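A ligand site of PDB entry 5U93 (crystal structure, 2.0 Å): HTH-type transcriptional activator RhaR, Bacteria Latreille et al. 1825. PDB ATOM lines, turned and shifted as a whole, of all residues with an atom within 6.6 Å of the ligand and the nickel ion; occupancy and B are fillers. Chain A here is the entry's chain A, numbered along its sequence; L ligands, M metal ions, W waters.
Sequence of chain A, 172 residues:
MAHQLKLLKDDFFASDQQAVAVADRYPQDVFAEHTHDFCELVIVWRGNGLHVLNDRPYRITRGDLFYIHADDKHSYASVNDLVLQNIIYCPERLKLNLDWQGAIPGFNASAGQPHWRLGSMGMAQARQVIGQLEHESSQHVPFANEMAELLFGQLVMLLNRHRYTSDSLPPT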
ATOM      1  N   LEU A   7      11.078  12.612 -19.059  1.00  0.00           N
ATOM      2  CA  LEU A   7      10.599  13.970 -18.862  1.00  0.00           C
ATOM      3  C   LEU A   7      11.112  14.567 -17.556  1.00  0.00           C
ATOM      4  O   LEU A   7      11.143  13.895 -16.516  1.00  0.00           O
ATOM      5  CB  LEU A   7       9.077  13.977 -18.878  1.00  0.00           C
ATOM      6  CG  LEU A   7       8.452  13.352 -20.119  1.00  0.00           C
ATOM      7  CD1 LEU A   7       6.944  13.557 -20.048  1.00  0.00           C
ATOM      8  CD2 LEU A   7       9.024  13.939 -21.399  1.00  0.00           C
ATOM      9  N   PHE A  12       8.675  21.051 -16.867  1.00  0.00           N
ATOM     10  CA  PHE A  12       7.241  20.957 -16.667  1.00  0.00           C
ATOM     11  C   PHE A  12       6.696  21.760 -15.477  1.00  0.00           C
ATOM     12  O   PHE A  12       5.494  21.990 -15.408  1.00  0.00           O
ATOM     13  CB  PHE A  12       6.780  19.483 -16.604  1.00  0.00           C
ATOM     14  CG  PHE A  12       6.785  18.806 -17.935  1.00  0.00           C
ATOM     15  CD1 PHE A  12       5.641  18.784 -18.717  1.00  0.00           C
ATOM     16  CD2 PHE A  12       7.952  18.257 -18.445  1.00  0.00           C
ATOM     17  CE1 PHE A  12       5.659  18.201 -19.989  1.00  0.00           C
ATOM     18  CE2 PHE A  12       7.984  17.674 -19.713  1.00  0.00           C
ATOM     19  CZ  PHE A  12       6.829  17.637 -20.482  1.00  0.00           C
ATOM     20  N   ALA A  23      -1.268  19.724 -16.006  1.00  0.00           N
ATOM     21  CA  ALA A  23      -1.044  19.685 -17.428  1.00  0.00           C
ATOM     22  C   ALA A  23      -2.290  19.135 -18.128  1.00  0.00           C
ATOM     23  O   ALA A  23      -2.589  17.929 -18.033  1.00  0.00           O
ATOM     24  CB  ALA A  23       0.160  18.822 -17.736  1.00  0.00           C
ATOM     25  N   ARG A  25      -4.552  17.837 -21.142  1.00  0.00           N
ATOM     26  CA  ARG A  25      -4.405  17.170 -22.425  1.00  0.00           C
ATOM     27  C   ARG A  25      -5.774  17.107 -23.094  1.00  0.00           C
ATOM     28  O   ARG A  25      -6.544  16.154 -22.876  1.00  0.00           O
ATOM     29  CB  ARG A  25      -3.797  15.783 -22.217  1.00  0.00           C
ATOM     30  CG  ARG A  25      -2.419  15.819 -21.533  1.00  0.00           C
ATOM     31  CD  ARG A  25      -1.378  16.484 -22.461  1.00  0.00           C
ATOM     32  NE  ARG A  25      -0.047  16.609 -21.864  1.00  0.00           N
ATOM     33  CZ  ARG A  25       0.445  17.733 -21.336  1.00  0.00           C
ATOM     34  NH1 ARG A  25      -0.284  18.836 -21.316  1.00  0.00           N
ATOM     35  NH2 ARG A  25       1.675  17.752 -20.834  1.00  0.00           N
ATOM     36  N   GLN A  28      -5.364  14.229 -25.348  1.00  0.00           N
ATOM     37  CA  GLN A  28      -4.067  13.551 -25.289  1.00  0.00           C
ATOM     38  C   GLN A  28      -3.856  12.831 -26.612  1.00  0.00           C
ATOM     39  O   GLN A  28      -4.643  11.964 -26.992  1.00  0.00           O
ATOM     40  CB  GLN A  28      -4.044  12.536 -24.146  1.00  0.00           C
ATOM     41  CG  GLN A  28      -2.794  11.658 -24.097  1.00  0.00           C
ATOM     42  CD  GLN A  28      -1.563  12.429 -23.619  1.00  0.00           C
ATOM     43  OE1 GLN A  28      -1.491  12.862 -22.463  1.00  0.00           O
ATOM     44  NE2 GLN A  28      -0.602  12.603 -24.520  1.00  0.00           N
ATOM     45  N   ASP A  29      -2.797  13.205 -27.322  1.00  0.00           N
ATOM     46  CA  ASP A  29      -2.445  12.516 -28.553  1.00  0.00           C
ATOM     47  C   ASP A  29      -1.539  11.338 -28.224  1.00  0.00           C
ATOM     48  O   ASP A  29      -1.190  11.110 -27.059  1.00  0.00           O
ATOM     49  CB  ASP A  29      -1.743  13.483 -29.511  1.00  0.00           C
ATOM     50  CG  ASP A  29      -2.573  14.739 -29.768  1.00  0.00           C
ATOM     51  OD1 ASP A  29      -3.566  14.644 -30.531  1.00  0.00           O
ATOM     52  OD2 ASP A  29      -2.232  15.816 -29.230  1.00  0.00           O
ATOM     53  N   PHE A  31       1.598   9.350 -27.541  1.00  0.00           N
ATOM     54  CA  PHE A  31       2.746   9.855 -26.805  1.00  0.00           C
ATOM     55  C   PHE A  31       3.709   8.716 -26.493  1.00  0.00           C
ATOM     56  O   PHE A  31       3.306   7.677 -25.972  1.00  0.00           O
ATOM     57  CB  PHE A  31       2.310  10.562 -25.520  1.00  0.00           C
ATOM     58  CG  PHE A  31       3.389  11.426 -24.926  1.00  0.00           C
ATOM     59  CD1 PHE A  31       4.221  10.927 -23.937  1.00  0.00           C
ATOM     60  CD2 PHE A  31       3.578  12.718 -25.370  1.00  0.00           C
ATOM     61  CE1 PHE A  31       5.221  11.735 -23.395  1.00  0.00           C
ATOM     62  CE2 PHE A  31       4.581  13.519 -24.841  1.00  0.00           C
ATOM     63  CZ  PHE A  31       5.399  13.022 -23.855  1.00  0.00           C
ATOM     64  N   HIS A  34       7.849   6.715 -22.006  1.00  0.00           N
ATOM     65  CA  HIS A  34       8.727   7.630 -21.286  1.00  0.00           C
ATOM     66  C   HIS A  34       8.678   7.384 -19.786  1.00  0.00           C
ATOM     67  O   HIS A  34       7.708   6.829 -19.257  1.00  0.00           O
ATOM     68  CB  HIS A  34       8.319   9.075 -21.556  1.00  0.00           C
ATOM     69  CG  HIS A  34       6.978   9.412 -21.012  1.00  0.00           C
ATOM     70  ND1 HIS A  34       5.801   9.098 -21.666  1.00  0.00           N
ATOM     71  CD2 HIS A  34       6.604   9.986 -19.839  1.00  0.00           C
ATOM     72  CE1 HIS A  34       4.773   9.475 -20.926  1.00  0.00           C
ATOM     73  NE2 HIS A  34       5.235  10.018 -19.821  1.00  0.00           N
ATOM     74  N   THR A  35       9.726   7.822 -19.108  1.00  0.00           N
ATOM     75  CA  THR A  35       9.708   7.921 -17.651  1.00  0.00           C
ATOM     76  C   THR A  35       9.789   9.393 -17.296  1.00  0.00           C
ATOM     77  O   THR A  35       9.707  10.258 -18.188  1.00  0.00           O
ATOM     78  CB  THR A  35      10.899   7.188 -17.019  1.00  0.00           C
ATOM     79  OG1 THR A  35      12.120   7.684 -17.581  1.00  0.00           O
ATOM     80  CG2 THR A  35      10.807   5.685 -17.304  1.00  0.00           C
ATOM     81  N   HIS A  36       9.969   9.688 -16.015  1.00  0.00           N
ATOM     82  CA  HIS A  36       9.934  11.054 -15.499  1.00  0.00           C
ATOM     83  C   HIS A  36      10.927  11.165 -14.356  1.00  0.00           C
ATOM     84  O   HIS A  36      11.439  10.160 -13.880  1.00  0.00           O
ATOM     85  CB  HIS A  36       8.542  11.404 -14.923  1.00  0.00           C
ATOM     86  CG  HIS A  36       7.376  10.769 -15.611  1.00  0.00           C
ATOM     87  ND1 HIS A  36       7.077   9.427 -15.495  1.00  0.00           N
ATOM     88  CD2 HIS A  36       6.384  11.305 -16.369  1.00  0.00           C
ATOM     89  CE1 HIS A  36       5.981   9.155 -16.171  1.00  0.00           C
ATOM     90  NE2 HIS A  36       5.544  10.281 -16.719  1.00  0.00           N
ATOM     91  N   PHE A  38       9.533  13.171 -11.977  1.00  0.00           N
ATOM     92  CA  PHE A  38       8.449  13.659 -11.120  1.00  0.00           C
ATOM     93  C   PHE A  38       7.349  12.612 -11.169  1.00  0.00           C
ATOM     94  O   PHE A  38       7.377  11.754 -12.054  1.00  0.00           O
ATOM     95  CB  PHE A  38       7.915  15.029 -11.594  1.00  0.00           C
ATOM     96  CG  PHE A  38       7.545  15.069 -13.063  1.00  0.00           C
ATOM     97  CD1 PHE A  38       6.240  14.746 -13.480  1.00  0.00           C
ATOM     98  CD2 PHE A  38       8.474  15.469 -14.022  1.00  0.00           C
ATOM     99  CE1 PHE A  38       5.897  14.799 -14.844  1.00  0.00           C
ATOM    100  CE2 PHE A  38       8.140  15.518 -15.391  1.00  0.00           C
ATOM    101  CZ  PHE A  38       6.837  15.179 -15.791  1.00  0.00           C
ATOM    102  N   GLU A  40       2.980  11.644 -11.177  1.00  0.00           N
ATOM    103  CA  GLU A  40       1.758  12.254 -11.703  1.00  0.00           C
ATOM    104  C   GLU A  40       0.495  11.448 -11.426  1.00  0.00           C
ATOM    105  O   GLU A  40       0.536  10.229 -11.329  1.00  0.00           O
ATOM    106  CB  GLU A  40       1.893  12.545 -13.217  1.00  0.00           C
ATOM    107  CG  GLU A  40       2.120  11.303 -14.058  1.00  0.00           C
ATOM    108  CD  GLU A  40       2.548  11.610 -15.481  1.00  0.00           C
ATOM    109  OE1 GLU A  40       3.129  12.689 -15.761  1.00  0.00           O
ATOM    110  OE2 GLU A  40       2.293  10.746 -16.338  1.00  0.00           O
ATOM    111  N   VAL A  42      -3.225  10.830 -13.109  1.00  0.00           N
ATOM    112  CA  VAL A  42      -3.909  10.957 -14.395  1.00  0.00           C
ATOM    113  C   VAL A  42      -5.398  10.737 -14.174  1.00  0.00           C
ATOM    114  O   VAL A  42      -5.801   9.721 -13.583  1.00  0.00           O
ATOM    115  CB  VAL A  42      -3.426   9.893 -15.381  1.00  0.00           C
ATOM    116  CG1 VAL A  42      -4.100  10.067 -16.729  1.00  0.00           C
ATOM    117  CG2 VAL A  42      -1.874   9.911 -15.485  1.00  0.00           C
ATOM    118  N   HIS A  51      -3.674   3.055 -22.729  1.00  0.00           N
ATOM    119  CA  HIS A  51      -2.601   3.461 -21.851  1.00  0.00           C
ATOM    120  C   HIS A  51      -1.753   2.229 -21.539  1.00  0.00           C
ATOM    121  O   HIS A  51      -2.246   1.276 -20.918  1.00  0.00           O
ATOM    122  CB  HIS A  51      -3.174   4.055 -20.567  1.00  0.00           C
ATOM    123  CG  HIS A  51      -2.140   4.454 -19.557  1.00  0.00           C
ATOM    124  ND1 HIS A  51      -2.371   4.396 -18.199  1.00  0.00           N
ATOM    125  CD2 HIS A  51      -0.891   4.954 -19.703  1.00  0.00           C
ATOM    126  CE1 HIS A  51      -1.294   4.826 -17.551  1.00  0.00           C
ATOM    127  NE2 HIS A  51      -0.390   5.170 -18.446  1.00  0.00           N
ATOM    128  N   ILE A  68       0.828   7.347 -11.027  1.00  0.00           N
ATOM    129  CA  ILE A  68       2.068   7.065 -11.749  1.00  0.00           C
ATOM    130  C   ILE A  68       3.270   7.525 -10.947  1.00  0.00           C
ATOM    131  O   ILE A  68       3.307   8.652 -10.462  1.00  0.00           O
ATOM    132  CB  ILE A  68       2.105   7.828 -13.090  1.00  0.00           C
ATOM    133  CG1 ILE A  68       0.800   7.626 -13.884  1.00  0.00           C
ATOM    134  CG2 ILE A  68       3.326   7.419 -13.920  1.00  0.00           C
ATOM    135  CD1 ILE A  68       0.578   6.219 -14.365  1.00  0.00           C
ATOM    136  N   ASP A  72       7.978   4.810 -13.446  1.00  0.00           N
ATOM    137  CA  ASP A  72       7.084   4.042 -14.311  1.00  0.00           C
ATOM    138  C   ASP A  72       7.335   4.472 -15.752  1.00  0.00           C
ATOM    139  O   ASP A  72       7.488   5.654 -16.042  1.00  0.00           O
ATOM    140  CB  ASP A  72       5.616   4.308 -13.958  1.00  0.00           C
ATOM    141  CG  ASP A  72       5.209   3.672 -12.651  1.00  0.00           C
ATOM    142  OD1 ASP A  72       5.822   2.665 -12.235  1.00  0.00           O
ATOM    143  OD2 ASP A  72       4.260   4.181 -12.028  1.00  0.00           O
ATOM    144  N   HIS A  74       5.581   4.630 -19.385  1.00  0.00           N
ATOM    145  CA  HIS A  74       4.228   4.540 -19.939  1.00  0.00           C
ATOM    146  C   HIS A  74       4.069   5.349 -21.206  1.00  0.00           C
ATOM    147  O   HIS A  74       4.926   6.183 -21.547  1.00  0.00           O
ATOM    148  CB  HIS A  74       3.148   4.874 -18.889  1.00  0.00           C
ATOM    149  CG  HIS A  74       3.084   6.316 -18.483  1.00  0.00           C
ATOM    150  ND1 HIS A  74       1.964   6.881 -17.923  1.00  0.00           N
ATOM    151  CD2 HIS A  74       4.014   7.309 -18.560  1.00  0.00           C
ATOM    152  CE1 HIS A  74       2.200   8.157 -17.662  1.00  0.00           C
ATOM    153  NE2 HIS A  74       3.433   8.446 -18.043  1.00  0.00           N
ATOM    154  N   SER A  75       2.979   5.074 -21.912  1.00  0.00           N
ATOM    155  CA  SER A  75       2.711   5.676 -23.206  1.00  0.00           C
ATOM    156  C   SER A  75       1.218   5.690 -23.503  1.00  0.00           C
ATOM    157  O   SER A  75       0.432   4.998 -22.865  1.00  0.00           O
ATOM    158  CB  SER A  75       3.443   4.904 -24.310  1.00  0.00           C
ATOM    159  OG  SER A  75       2.908   3.604 -24.448  1.00  0.00           O
ATOM    160  N   TYR A  76       0.836   6.488 -24.501  1.00  0.00           N
ATOM    161  CA  TYR A  76      -0.528   6.542 -24.970  1.00  0.00           C
ATOM    162  C   TYR A  76      -0.544   6.242 -26.460  1.00  0.00           C
ATOM    163  O   TYR A  76       0.218   6.828 -27.208  1.00  0.00           O
ATOM    164  CB  TYR A  76      -1.122   7.917 -24.708  1.00  0.00           C
ATOM    165  CG  TYR A  76      -1.241   8.195 -23.243  1.00  0.00           C
ATOM    166  CD1 TYR A  76      -0.278   8.940 -22.587  1.00  0.00           C
ATOM    167  CD2 TYR A  76      -2.287   7.676 -22.504  1.00  0.00           C
ATOM    168  CE1 TYR A  76      -0.375   9.191 -21.216  1.00  0.00           C
ATOM    169  CE2 TYR A  76      -2.397   7.912 -21.145  1.00  0.00           C
ATOM    170  CZ  TYR A  76      -1.429   8.669 -20.510  1.00  0.00           C
ATOM    171  OH  TYR A  76      -1.510   8.913 -19.149  1.00  0.00           O
ATOM    172  N   LEU A  84      -7.843  14.131 -20.942  1.00  0.00           N
ATOM    173  CA  LEU A  84      -7.364  13.831 -19.600  1.00  0.00           C
ATOM    174  C   LEU A  84      -6.602  14.999 -19.001  1.00  0.00           C
ATOM    175  O   LEU A  84      -6.334  15.987 -19.676  1.00  0.00           O
ATOM    176  CB  LEU A  84      -6.515  12.543 -19.590  1.00  0.00           C
ATOM    177  CG  LEU A  84      -5.197  12.439 -20.381  1.00  0.00           C
ATOM    178  CD1 LEU A  84      -4.052  13.110 -19.650  1.00  0.00           C
ATOM    179  CD2 LEU A  84      -4.862  10.984 -20.645  1.00  0.00           C
ATOM    180  N   ASN A  86      -3.157  15.626 -16.374  1.00  0.00           N
ATOM    181  CA  ASN A  86      -2.091  15.134 -15.520  1.00  0.00           C
ATOM    182  C   ASN A  86      -1.899  16.118 -14.389  1.00  0.00           C
ATOM    183  O   ASN A  86      -1.651  17.292 -14.615  1.00  0.00           O
ATOM    184  CB  ASN A  86      -0.765  15.018 -16.287  1.00  0.00           C
ATOM    185  CG  ASN A  86      -0.824  14.008 -17.401  1.00  0.00           C
ATOM    186  OD1 ASN A  86      -1.107  12.839 -17.177  1.00  0.00           O
ATOM    187  ND2 ASN A  86      -0.536  14.460 -18.620  1.00  0.00           N
ATOM    188  N   ILE A  88       0.750  16.765 -12.029  1.00  0.00           N
ATOM    189  CA  ILE A  88       2.147  16.375 -11.824  1.00  0.00           C
ATOM    190  C   ILE A  88       2.652  16.976 -10.514  1.00  0.00           C
ATOM    191  O   ILE A  88       2.275  18.079 -10.132  1.00  0.00           O
ATOM    192  CB  ILE A  88       3.024  16.793 -13.020  1.00  0.00           C
ATOM    193  CG1 ILE A  88       3.040  18.315 -13.190  1.00  0.00           C
ATOM    194  CG2 ILE A  88       2.496  16.139 -14.308  1.00  0.00           C
ATOM    195  CD1 ILE A  88       3.977  18.802 -14.313  1.00  0.00           C
HETATM  196  C1  LIG L   1       2.503  13.994 -21.572  1.00  0.00           C
HETATM  197  C2  LIG L   1       1.993  12.662 -21.139  1.00  0.00           C
HETATM  198  C3  LIG L   1       2.823  12.105 -20.063  1.00  0.00           C
HETATM  199  C4  LIG L   1       3.046  13.017 -18.930  1.00  0.00           C
HETATM  200  C5  LIG L   1       3.497  14.383 -19.385  1.00  0.00           C
HETATM  201  C6  LIG L   1       3.433  15.329 -18.261  1.00  0.00           C
HETATM  202  O1  LIG L   1       1.683  14.544 -22.473  1.00  0.00           O
HETATM  203  O2  LIG L   1       0.639  12.771 -20.722  1.00  0.00           O
HETATM  204  O3  LIG L   1       2.260  10.886 -19.554  1.00  0.00           O
HETATM  205  O4  LIG L   1       3.984  12.426 -18.050  1.00  0.00           O
HETATM  206  O5  LIG L   1       2.658  14.911 -20.431  1.00  0.00           O
HETATM  207 NI    NI M   1       3.889  10.371 -18.057  1.00  0.00          NI
HETATM  208  O   HOH W   1       0.139  10.752 -18.121  1.00  0.00           O
HETATM  209  O   HOH W   2       3.767  16.693 -23.119  1.00  0.00           O
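An oxygen (O2) of the ligand lies within hydrogen-bond range of the side-chain amide oxygen (OE1) of Gln 28, at 2.8 Å. An oxygen (O1) of the ligand lies within hydrogen-bond range of the guanidinium group (NE) of Arg 25 (2.8 Å). ND2 of Asn 86 lies within hydrogen-bond range of O2 of the ligand.
Merely in contact with the ligand: Tyr 76, Leu 7 and Phe 31. Hydrophobic or aromatic side chains that line the ligand: Leu 7, Phe 31, His 34, His 36, His 74 and Tyr 76.
Four residues have an atom within 4 Å of the nickel ion: His 34, His 36, Glu 40 and His 74. Along chain A the residues within 4 Å of the nickel ion span positions 34 to 74. The nearest printed residue that does not touch the nickel ion is Leu 7 (4.8 Å).
The nickel ion is bound by NE2 of His 74 (2.0 Å). An oxygen (O4) of the ligand is bound to the nickel ion (2.1 Å). NE2 of His 36 is bound to the nickel ion. NE2 of His 34 binds the nickel ion, 2.2 Å away. The nickel ion is bound by O3 of the ligand (2.3 Å). The nickel ion is bound by the side-chain carboxylate (OE2) of Glu 40.
ND1 of His 74 is in hydrogen-bond range of NE2 of His 51. The backbone NH (N) of Ile 68 sits at hydrogen-bond distance from the backbone carbonyl oxygen (O) of Glu 40 (2.9 Å). The backbone NH (N) of Arg 25 lies within hydrogen-bond range of the backbone carbonyl oxygen (O) of Leu 84 (3.0 Å). N of Ala 23 lies within hydrogen-bond range of O of Asn 86 (2.8 Å). The backbone NH of Phe 31 is in hydrogen-bond range of the backbone carbonyl oxygen of Tyr 76. N of Leu 7 is in hydrogen-bond range of O of Thr 35, 2.9 Å away.
Water W1 lies within hydrogen-bond range of OD1 of Asn 86 (2.6 Å), OH of Tyr 76 (2.7 Å) and O2 of the ligand (3.3 Å). Water W2 bridges O1 of the ligand (3.1 Å) and NH2 of Arg 25 (3.3 Å).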
